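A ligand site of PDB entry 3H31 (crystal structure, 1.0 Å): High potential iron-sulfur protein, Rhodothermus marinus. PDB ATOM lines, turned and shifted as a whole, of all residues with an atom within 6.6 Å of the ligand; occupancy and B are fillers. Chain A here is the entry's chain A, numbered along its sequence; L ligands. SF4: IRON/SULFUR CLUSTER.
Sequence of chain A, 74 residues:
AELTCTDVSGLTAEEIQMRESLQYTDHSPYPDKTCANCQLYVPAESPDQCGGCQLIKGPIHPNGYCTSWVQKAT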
ATOM      1  N   LEU A  22     -18.947 -36.505 -20.217  1.00  0.00           N
ATOM      2  CA  LEU A  22     -18.764 -35.094 -19.956  1.00  0.00           C
ATOM      3  C   LEU A  22     -19.503 -34.185 -20.908  1.00  0.00           C
ATOM      4  O   LEU A  22     -19.382 -32.956 -20.863  1.00  0.00           O
ATOM      5  CB  LEU A  22     -17.272 -34.769 -19.874  1.00  0.00           C
ATOM      6  CG  LEU A  22     -16.517 -35.530 -18.769  1.00  0.00           C
ATOM      7  CD1 LEU A  22     -15.028 -35.191 -18.825  1.00  0.00           C
ATOM      8  CD2 LEU A  22     -17.109 -35.259 -17.378  1.00  0.00           C
ATOM      9  N   TYR A  24     -19.168 -33.599 -24.123  1.00  0.00           N
ATOM     10  CA  TYR A  24     -18.369 -32.790 -25.041  1.00  0.00           C
ATOM     11  C   TYR A  24     -19.253 -32.373 -26.241  1.00  0.00           C
ATOM     12  O   TYR A  24     -19.896 -33.219 -26.850  1.00  0.00           O
ATOM     13  CB  TYR A  24     -17.053 -33.552 -25.509  1.00  0.00           C
ATOM     14  CG  TYR A  24     -16.463 -32.641 -26.594  1.00  0.00           C
ATOM     15  CD1 TYR A  24     -15.766 -31.486 -26.230  1.00  0.00           C
ATOM     16  CD2 TYR A  24     -16.689 -32.865 -27.961  1.00  0.00           C
ATOM     17  CE1 TYR A  24     -15.279 -30.613 -27.183  1.00  0.00           C
ATOM     18  CE2 TYR A  24     -16.274 -31.957 -28.883  1.00  0.00           C
ATOM     19  CZ  TYR A  24     -15.553 -30.864 -28.544  1.00  0.00           C
ATOM     20  OH  TYR A  24     -15.167 -29.947 -29.448  1.00  0.00           O
ATOM     21  N   LYS A  33     -18.480 -19.855 -21.466  1.00  0.00           N
ATOM     22  CA  LYS A  33     -17.694 -21.004 -21.088  1.00  0.00           C
ATOM     23  C   LYS A  33     -17.446 -21.819 -22.349  1.00  0.00           C
ATOM     24  O   LYS A  33     -18.345 -22.454 -22.876  1.00  0.00           O
ATOM     25  CB  LYS A  33     -18.387 -21.868 -20.034  1.00  0.00           C
ATOM     26  CG  LYS A  33     -18.646 -21.139 -18.731  1.00  0.00           C
ATOM     27  CD  LYS A  33     -19.371 -22.092 -17.774  1.00  0.00           C
ATOM     28  CE  LYS A  33     -20.210 -21.366 -16.730  1.00  0.00           C
ATOM     29  NZ  LYS A  33     -21.301 -22.297 -16.300  1.00  0.00           N
ATOM     30  N   THR A  34     -16.186 -21.773 -22.836  1.00  0.00           N
ATOM     31  CA  THR A  34     -15.803 -22.565 -23.981  1.00  0.00           C
ATOM     32  C   THR A  34     -14.445 -23.210 -23.693  1.00  0.00           C
ATOM     33  O   THR A  34     -13.737 -22.775 -22.781  1.00  0.00           O
ATOM     34  CB  THR A  34     -15.700 -21.758 -25.309  1.00  0.00           C
ATOM     35  OG1 THR A  34     -14.630 -20.826 -25.213  1.00  0.00           O
ATOM     36  CG2 THR A  34     -17.019 -21.070 -25.644  1.00  0.00           C
ATOM     37  N   CYS A  35     -14.063 -24.134 -24.543  1.00  0.00           N
ATOM     38  CA  CYS A  35     -12.730 -24.718 -24.335  1.00  0.00           C
ATOM     39  C   CYS A  35     -11.677 -23.645 -24.393  1.00  0.00           C
ATOM     40  O   CYS A  35     -10.696 -23.691 -23.628  1.00  0.00           O
ATOM     41  CB  CYS A  35     -12.487 -25.796 -25.404  1.00  0.00           C
ATOM     42  SG  CYS A  35     -13.646 -27.171 -25.290  1.00  0.00           S
ATOM     43  N   ALA A  36     -11.816 -22.642 -25.252  1.00  0.00           N
ATOM     44  CA  ALA A  36     -10.788 -21.614 -25.342  1.00  0.00           C
ATOM     45  C   ALA A  36     -10.610 -20.824 -24.056  1.00  0.00           C
ATOM     46  O   ALA A  36      -9.567 -20.143 -23.918  1.00  0.00           O
ATOM     47  CB  ALA A  36     -11.069 -20.665 -26.499  1.00  0.00           C
ATOM     48  N   CYS A  38     -10.981 -22.359 -20.974  1.00  0.00           N
ATOM     49  CA  CYS A  38     -10.821 -23.439 -20.011  1.00  0.00           C
ATOM     50  C   CYS A  38      -9.316 -23.711 -19.745  1.00  0.00           C
ATOM     51  O   CYS A  38      -8.503 -23.712 -20.652  1.00  0.00           O
ATOM     52  CB  CYS A  38     -11.433 -24.733 -20.565  1.00  0.00           C
ATOM     53  SG  CYS A  38     -11.252 -26.163 -19.471  1.00  0.00           S
ATOM     54  N   GLN A  39      -8.982 -24.001 -18.473  1.00  0.00           N
ATOM     55  CA  GLN A  39      -7.593 -24.227 -18.138  1.00  0.00           C
ATOM     56  C   GLN A  39      -7.051 -25.479 -18.778  1.00  0.00           C
ATOM     57  O   GLN A  39      -5.815 -25.596 -18.842  1.00  0.00           O
ATOM     58  CB  GLN A  39      -7.399 -24.361 -16.632  1.00  0.00           C
ATOM     59  CG  GLN A  39      -7.522 -23.173 -15.718  1.00  0.00           C
ATOM     60  CD  GLN A  39      -7.152 -23.473 -14.270  1.00  0.00           C
ATOM     61  OE1 GLN A  39      -6.490 -24.451 -13.993  1.00  0.00           O
ATOM     62  NE2 GLN A  39      -7.594 -22.718 -13.312  1.00  0.00           N
ATOM     63  N   LEU A  40      -7.868 -26.432 -19.235  1.00  0.00           N
ATOM     64  CA  LEU A  40      -7.359 -27.703 -19.716  1.00  0.00           C
ATOM     65  C   LEU A  40      -7.209 -27.765 -21.228  1.00  0.00           C
ATOM     66  O   LEU A  40      -6.729 -28.777 -21.775  1.00  0.00           O
ATOM     67  CB  LEU A  40      -8.240 -28.849 -19.200  1.00  0.00           C
ATOM     68  CG  LEU A  40      -8.280 -28.916 -17.660  1.00  0.00           C
ATOM     69  CD1 LEU A  40      -9.152 -30.051 -17.184  1.00  0.00           C
ATOM     70  CD2 LEU A  40      -6.927 -29.059 -17.035  1.00  0.00           C
ATOM     71  N   TYR A  41      -7.507 -26.653 -21.922  1.00  0.00           N
ATOM     72  CA  TYR A  41      -7.449 -26.627 -23.380  1.00  0.00           C
ATOM     73  C   TYR A  41      -6.013 -26.448 -23.870  1.00  0.00           C
ATOM     74  O   TYR A  41      -5.222 -25.692 -23.267  1.00  0.00           O
ATOM     75  CB  TYR A  41      -8.320 -25.489 -23.906  1.00  0.00           C
ATOM     76  CG  TYR A  41      -8.434 -25.438 -25.401  1.00  0.00           C
ATOM     77  CD1 TYR A  41      -8.968 -26.522 -26.085  1.00  0.00           C
ATOM     78  CD2 TYR A  41      -8.047 -24.318 -26.133  1.00  0.00           C
ATOM     79  CE1 TYR A  41      -9.075 -26.500 -27.467  1.00  0.00           C
ATOM     80  CE2 TYR A  41      -8.143 -24.289 -27.533  1.00  0.00           C
ATOM     81  CZ  TYR A  41      -8.670 -25.376 -28.187  1.00  0.00           C
ATOM     82  OH  TYR A  41      -8.776 -25.441 -29.568  1.00  0.00           O
ATOM     83  N   VAL A  42      -5.693 -27.102 -24.954  1.00  0.00           N
ATOM     84  CA  VAL A  42      -4.430 -26.942 -25.643  1.00  0.00           C
ATOM     85  C   VAL A  42      -4.712 -26.449 -27.052  1.00  0.00           C
ATOM     86  O   VAL A  42      -5.234 -27.208 -27.852  1.00  0.00           O
ATOM     87  CB  VAL A  42      -3.659 -28.276 -25.673  1.00  0.00           C
ATOM     88  CG1 VAL A  42      -2.294 -28.059 -26.377  1.00  0.00           C
ATOM     89  CG2 VAL A  42      -3.449 -28.782 -24.267  1.00  0.00           C
ATOM     90  N   GLY A  52      -6.818 -29.582 -28.571  1.00  0.00           N
ATOM     91  CA  GLY A  52      -6.865 -30.764 -27.715  1.00  0.00           C
ATOM     92  C   GLY A  52      -7.160 -30.364 -26.318  1.00  0.00           C
ATOM     93  O   GLY A  52      -7.318 -29.175 -25.978  1.00  0.00           O
ATOM     94  N   CYS A  53      -7.231 -31.363 -25.450  1.00  0.00           N
ATOM     95  CA  CYS A  53      -7.605 -31.191 -24.061  1.00  0.00           C
ATOM     96  C   CYS A  53      -6.781 -32.140 -23.205  1.00  0.00           C
ATOM     97  O   CYS A  53      -6.482 -33.268 -23.619  1.00  0.00           O
ATOM     98  CB  CYS A  53      -9.108 -31.501 -23.903  1.00  0.00           C
ATOM     99  SG  CYS A  53      -9.703 -31.481 -22.205  1.00  0.00           S
ATOM    100  N   GLN A  54      -6.402 -31.670 -22.026  1.00  0.00           N
ATOM    101  CA  GLN A  54      -5.642 -32.473 -21.087  1.00  0.00           C
ATOM    102  C   GLN A  54      -6.499 -33.559 -20.447  1.00  0.00           C
ATOM    103  O   GLN A  54      -5.950 -34.506 -19.858  1.00  0.00           O
ATOM    104  CB  GLN A  54      -5.164 -31.639 -19.912  1.00  0.00           C
ATOM    105  CG  GLN A  54      -3.993 -30.749 -20.156  1.00  0.00           C
ATOM    106  CD  GLN A  54      -3.438 -30.363 -18.790  1.00  0.00           C
ATOM    107  OE1 GLN A  54      -3.334 -31.023 -17.715  1.00  0.00           O
ATOM    108  NE2 GLN A  54      -2.921 -29.169 -18.610  1.00  0.00           N
ATOM    109  N   LEU A  55      -7.806 -33.416 -20.480  1.00  0.00           N
ATOM    110  CA  LEU A  55      -8.765 -34.294 -19.815  1.00  0.00           C
ATOM    111  C   LEU A  55      -9.400 -35.300 -20.754  1.00  0.00           C
ATOM    112  O   LEU A  55      -9.431 -36.495 -20.480  1.00  0.00           O
ATOM    113  CB  LEU A  55      -9.833 -33.449 -19.124  1.00  0.00           C
ATOM    114  CG  LEU A  55     -10.582 -34.152 -18.003  1.00  0.00           C
ATOM    115  CD1 LEU A  55      -9.676 -34.321 -16.773  1.00  0.00           C
ATOM    116  CD2 LEU A  55     -11.806 -33.353 -17.626  1.00  0.00           C
ATOM    117  N   ILE A  56      -9.931 -34.849 -21.862  1.00  0.00           N
ATOM    118  CA  ILE A  56     -10.495 -35.861 -22.751  1.00  0.00           C
ATOM    119  C   ILE A  56      -9.748 -35.827 -24.074  1.00  0.00           C
ATOM    120  O   ILE A  56      -9.095 -34.872 -24.486  1.00  0.00           O
ATOM    121  CB  ILE A  56     -11.987 -35.593 -22.978  1.00  0.00           C
ATOM    122  CG1 ILE A  56     -12.206 -34.266 -23.652  1.00  0.00           C
ATOM    123  CG2 ILE A  56     -12.712 -35.651 -21.656  1.00  0.00           C
ATOM    124  CD1 ILE A  56     -13.655 -33.962 -23.987  1.00  0.00           C
ATOM    125  N   ILE A  60     -10.644 -31.294 -30.307  1.00  0.00           N
ATOM    126  CA  ILE A  60     -11.399 -30.423 -29.430  1.00  0.00           C
ATOM    127  C   ILE A  60     -11.519 -29.061 -30.059  1.00  0.00           C
ATOM    128  O   ILE A  60     -10.515 -28.447 -30.492  1.00  0.00           O
ATOM    129  CB  ILE A  60     -10.742 -30.265 -28.042  1.00  0.00           C
ATOM    130  CG1 ILE A  60     -10.503 -31.639 -27.368  1.00  0.00           C
ATOM    131  CG2 ILE A  60     -11.506 -29.320 -27.125  1.00  0.00           C
ATOM    132  CD1 ILE A  60     -11.759 -32.302 -26.830  1.00  0.00           C
ATOM    133  N   HIS A  61     -12.766 -28.525 -30.202  1.00  0.00           N
ATOM    134  CA  HIS A  61     -12.988 -27.240 -30.827  1.00  0.00           C
ATOM    135  C   HIS A  61     -12.846 -26.109 -29.827  1.00  0.00           C
ATOM    136  O   HIS A  61     -13.396 -26.212 -28.703  1.00  0.00           O
ATOM    137  CB  HIS A  61     -14.403 -27.236 -31.389  1.00  0.00           C
ATOM    138  CG  HIS A  61     -14.638 -26.180 -32.412  1.00  0.00           C
ATOM    139  ND1 HIS A  61     -14.670 -24.811 -32.126  1.00  0.00           N
ATOM    140  CD2 HIS A  61     -14.805 -26.354 -33.768  1.00  0.00           C
ATOM    141  CE1 HIS A  61     -14.840 -24.204 -33.266  1.00  0.00           C
ATOM    142  NE2 HIS A  61     -14.940 -25.096 -34.270  1.00  0.00           N
ATOM    143  N   GLY A  64     -16.021 -25.187 -28.164  1.00  0.00           N
ATOM    144  CA  GLY A  64     -16.699 -26.304 -27.560  1.00  0.00           C
ATOM    145  C   GLY A  64     -16.818 -26.168 -26.044  1.00  0.00           C
ATOM    146  O   GLY A  64     -16.569 -25.125 -25.468  1.00  0.00           O
ATOM    147  N   TYR A  65     -17.262 -27.263 -25.430  1.00  0.00           N
ATOM    148  CA  TYR A  65     -17.484 -27.295 -24.001  1.00  0.00           C
ATOM    149  C   TYR A  65     -17.614 -28.746 -23.561  1.00  0.00           C
ATOM    150  O   TYR A  65     -18.090 -29.605 -24.317  1.00  0.00           O
ATOM    151  CB  TYR A  65     -18.794 -26.546 -23.677  1.00  0.00           C
ATOM    152  CG  TYR A  65     -19.263 -26.647 -22.252  1.00  0.00           C
ATOM    153  CD1 TYR A  65     -18.775 -25.803 -21.282  1.00  0.00           C
ATOM    154  CD2 TYR A  65     -20.237 -27.569 -21.893  1.00  0.00           C
ATOM    155  CE1 TYR A  65     -19.196 -25.850 -19.945  1.00  0.00           C
ATOM    156  CE2 TYR A  65     -20.695 -27.664 -20.591  1.00  0.00           C
ATOM    157  CZ  TYR A  65     -20.142 -26.777 -19.625  1.00  0.00           C
ATOM    158  OH  TYR A  65     -20.609 -26.924 -18.294  1.00  0.00           O
ATOM    159  N   CYS A  66     -17.257 -28.993 -22.303  1.00  0.00           N
ATOM    160  CA  CYS A  66     -17.670 -30.193 -21.590  1.00  0.00           C
ATOM    161  C   CYS A  66     -17.975 -29.753 -20.139  1.00  0.00           C
ATOM    162  O   CYS A  66     -17.563 -28.670 -19.720  1.00  0.00           O
ATOM    163  CB  CYS A  66     -16.691 -31.361 -21.630  1.00  0.00           C
ATOM    164  SG  CYS A  66     -15.357 -31.260 -20.402  1.00  0.00           S
ATOM    165  N   THR A  67     -18.644 -30.638 -19.392  1.00  0.00           N
ATOM    166  CA  THR A  67     -19.080 -30.233 -18.038  1.00  0.00           C
ATOM    167  C   THR A  67     -17.943 -30.130 -17.053  1.00  0.00           C
ATOM    168  O   THR A  67     -18.185 -29.595 -15.945  1.00  0.00           O
ATOM    169  CB  THR A  67     -20.184 -31.121 -17.519  1.00  0.00           C
ATOM    170  OG1 THR A  67     -19.740 -32.500 -17.481  1.00  0.00           O
ATOM    171  CG2 THR A  67     -21.428 -31.002 -18.395  1.00  0.00           C
ATOM    172  N   SER A  68     -16.755 -30.552 -17.400  1.00  0.00           N
ATOM    173  CA  SER A  68     -15.589 -30.373 -16.539  1.00  0.00           C
ATOM    174  C   SER A  68     -14.861 -29.054 -16.766  1.00  0.00           C
ATOM    175  O   SER A  68     -13.831 -28.847 -16.068  1.00  0.00           O
ATOM    176  CB  SER A  68     -14.553 -31.455 -16.649  1.00  0.00           C
ATOM    177  OG  SER A  68     -15.134 -32.697 -16.348  1.00  0.00           O
ATOM    178  N   TRP A  69     -15.372 -28.170 -17.587  1.00  0.00           N
ATOM    179  CA  TRP A  69     -14.796 -26.840 -17.852  1.00  0.00           C
ATOM    180  C   TRP A  69     -14.237 -26.238 -16.548  1.00  0.00           C
ATOM    181  O   TRP A  69     -14.935 -26.175 -15.547  1.00  0.00           O
ATOM    182  CB  TRP A  69     -15.888 -25.953 -18.452  1.00  0.00           C
ATOM    183  CG  TRP A  69     -15.450 -24.589 -18.797  1.00  0.00           C
ATOM    184  CD1 TRP A  69     -14.907 -24.163 -19.944  1.00  0.00           C
ATOM    185  CD2 TRP A  69     -15.536 -23.414 -17.975  1.00  0.00           C
ATOM    186  NE1 TRP A  69     -14.607 -22.851 -19.914  1.00  0.00           N
ATOM    187  CE2 TRP A  69     -15.015 -22.314 -18.706  1.00  0.00           C
ATOM    188  CE3 TRP A  69     -16.031 -23.178 -16.678  1.00  0.00           C
ATOM    189  CZ2 TRP A  69     -14.968 -21.060 -18.186  1.00  0.00           C
ATOM    190  CZ3 TRP A  69     -15.984 -21.864 -16.135  1.00  0.00           C
ATOM    191  CH2 TRP A  69     -15.442 -20.839 -16.948  1.00  0.00           C
ATOM    192  N   VAL A  70     -12.969 -25.824 -16.648  1.00  0.00           N
ATOM    193  CA  VAL A  70     -12.222 -25.289 -15.515  1.00  0.00           C
ATOM    194  C   VAL A  70     -11.922 -23.831 -15.813  1.00  0.00           C
ATOM    195  O   VAL A  70     -11.159 -23.491 -16.740  1.00  0.00           O
ATOM    196  CB  VAL A  70     -10.906 -26.068 -15.271  1.00  0.00           C
ATOM    197  CG1 VAL A  70     -10.104 -25.417 -14.149  1.00  0.00           C
ATOM    198  CG2 VAL A  70     -11.118 -27.549 -14.990  1.00  0.00           C
HETATM  199 FE1  SF4 L   1     -11.400 -29.985 -22.204  1.00  0.00          FE
HETATM  200 FE2  SF4 L   1     -13.110 -28.193 -23.352  1.00  0.00          FE
HETATM  201 FE3  SF4 L   1     -13.914 -29.747 -21.269  1.00  0.00          FE
HETATM  202 FE4  SF4 L   1     -12.078 -27.796 -20.814  1.00  0.00          FE
HETATM  203  S1  SF4 L   1     -14.289 -27.511 -21.473  1.00  0.00           S
HETATM  204  S2  SF4 L   1     -12.022 -29.860 -19.977  1.00  0.00           S
HETATM  205  S3  SF4 L   1     -10.888 -27.888 -22.798  1.00  0.00           S
HETATM  206  S4  SF4 L   1     -13.324 -30.422 -23.413  1.00  0.00           S
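SG of Cys 35 binds FE2 of the ligand, 2.3 Å away.
The side-chain sulfur (SG) of Cys 53 is bound to an iron atom (FE1) of the ligand.
The backbone NH (N) of Cys 66 sits close to a sulfur (S1) of the ligand (3.4 Å).
The side-chain sulfur (SG) of Cys 66 binds an iron atom (FE3) of the ligand.
The side-chain sulfur (SG) of Cys 38 is bound to an iron atom (FE4) of the ligand (2.3 Å).
N of Tyr 41 sits close to S3 of the ligand (3.7 Å).
N of Tyr 65 sits close to SG of Cys 35 (3.6 Å).
O of Gly 64 lies within hydrogen-bond range of N of Cys 35 (2.8 Å).
SG of Cys 35 sits close to O of His 61, at 3.6 Å.
The backbone NH (N) of Ile 56 lies close to the side-chain sulfur (SG) of Cys 53.
The side-chain sulfur (SG) of Cys 53 sits close to the backbone NH (N) of Leu 55, at 3.2 Å.
The side-chain sulfur of Cys 66 lies close to the backbone NH of Ser 68.
The backbone NH of His 61 lies within hydrogen-bond range of the side-chain hydroxyl of Tyr 24 (2.9 Å).
N of Gln 54 lies within hydrogen-bond range of O of Leu 40 (2.9 Å).
Residues that only touch the ligand: Tyr 24, Leu 40, Ile 56 and Trp 69.
Hydrophobic or aromatic side chains within 4 Å of the ligand: Tyr 24, Leu 40, Tyr 41, Ile 56 and Trp 69.
Within 4 Å of the ligand: Tyr 24, Cys 35, Cys 38, Leu 40, Tyr 41, Cys 53, Ile 56, Cys 66 and Trp 69.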
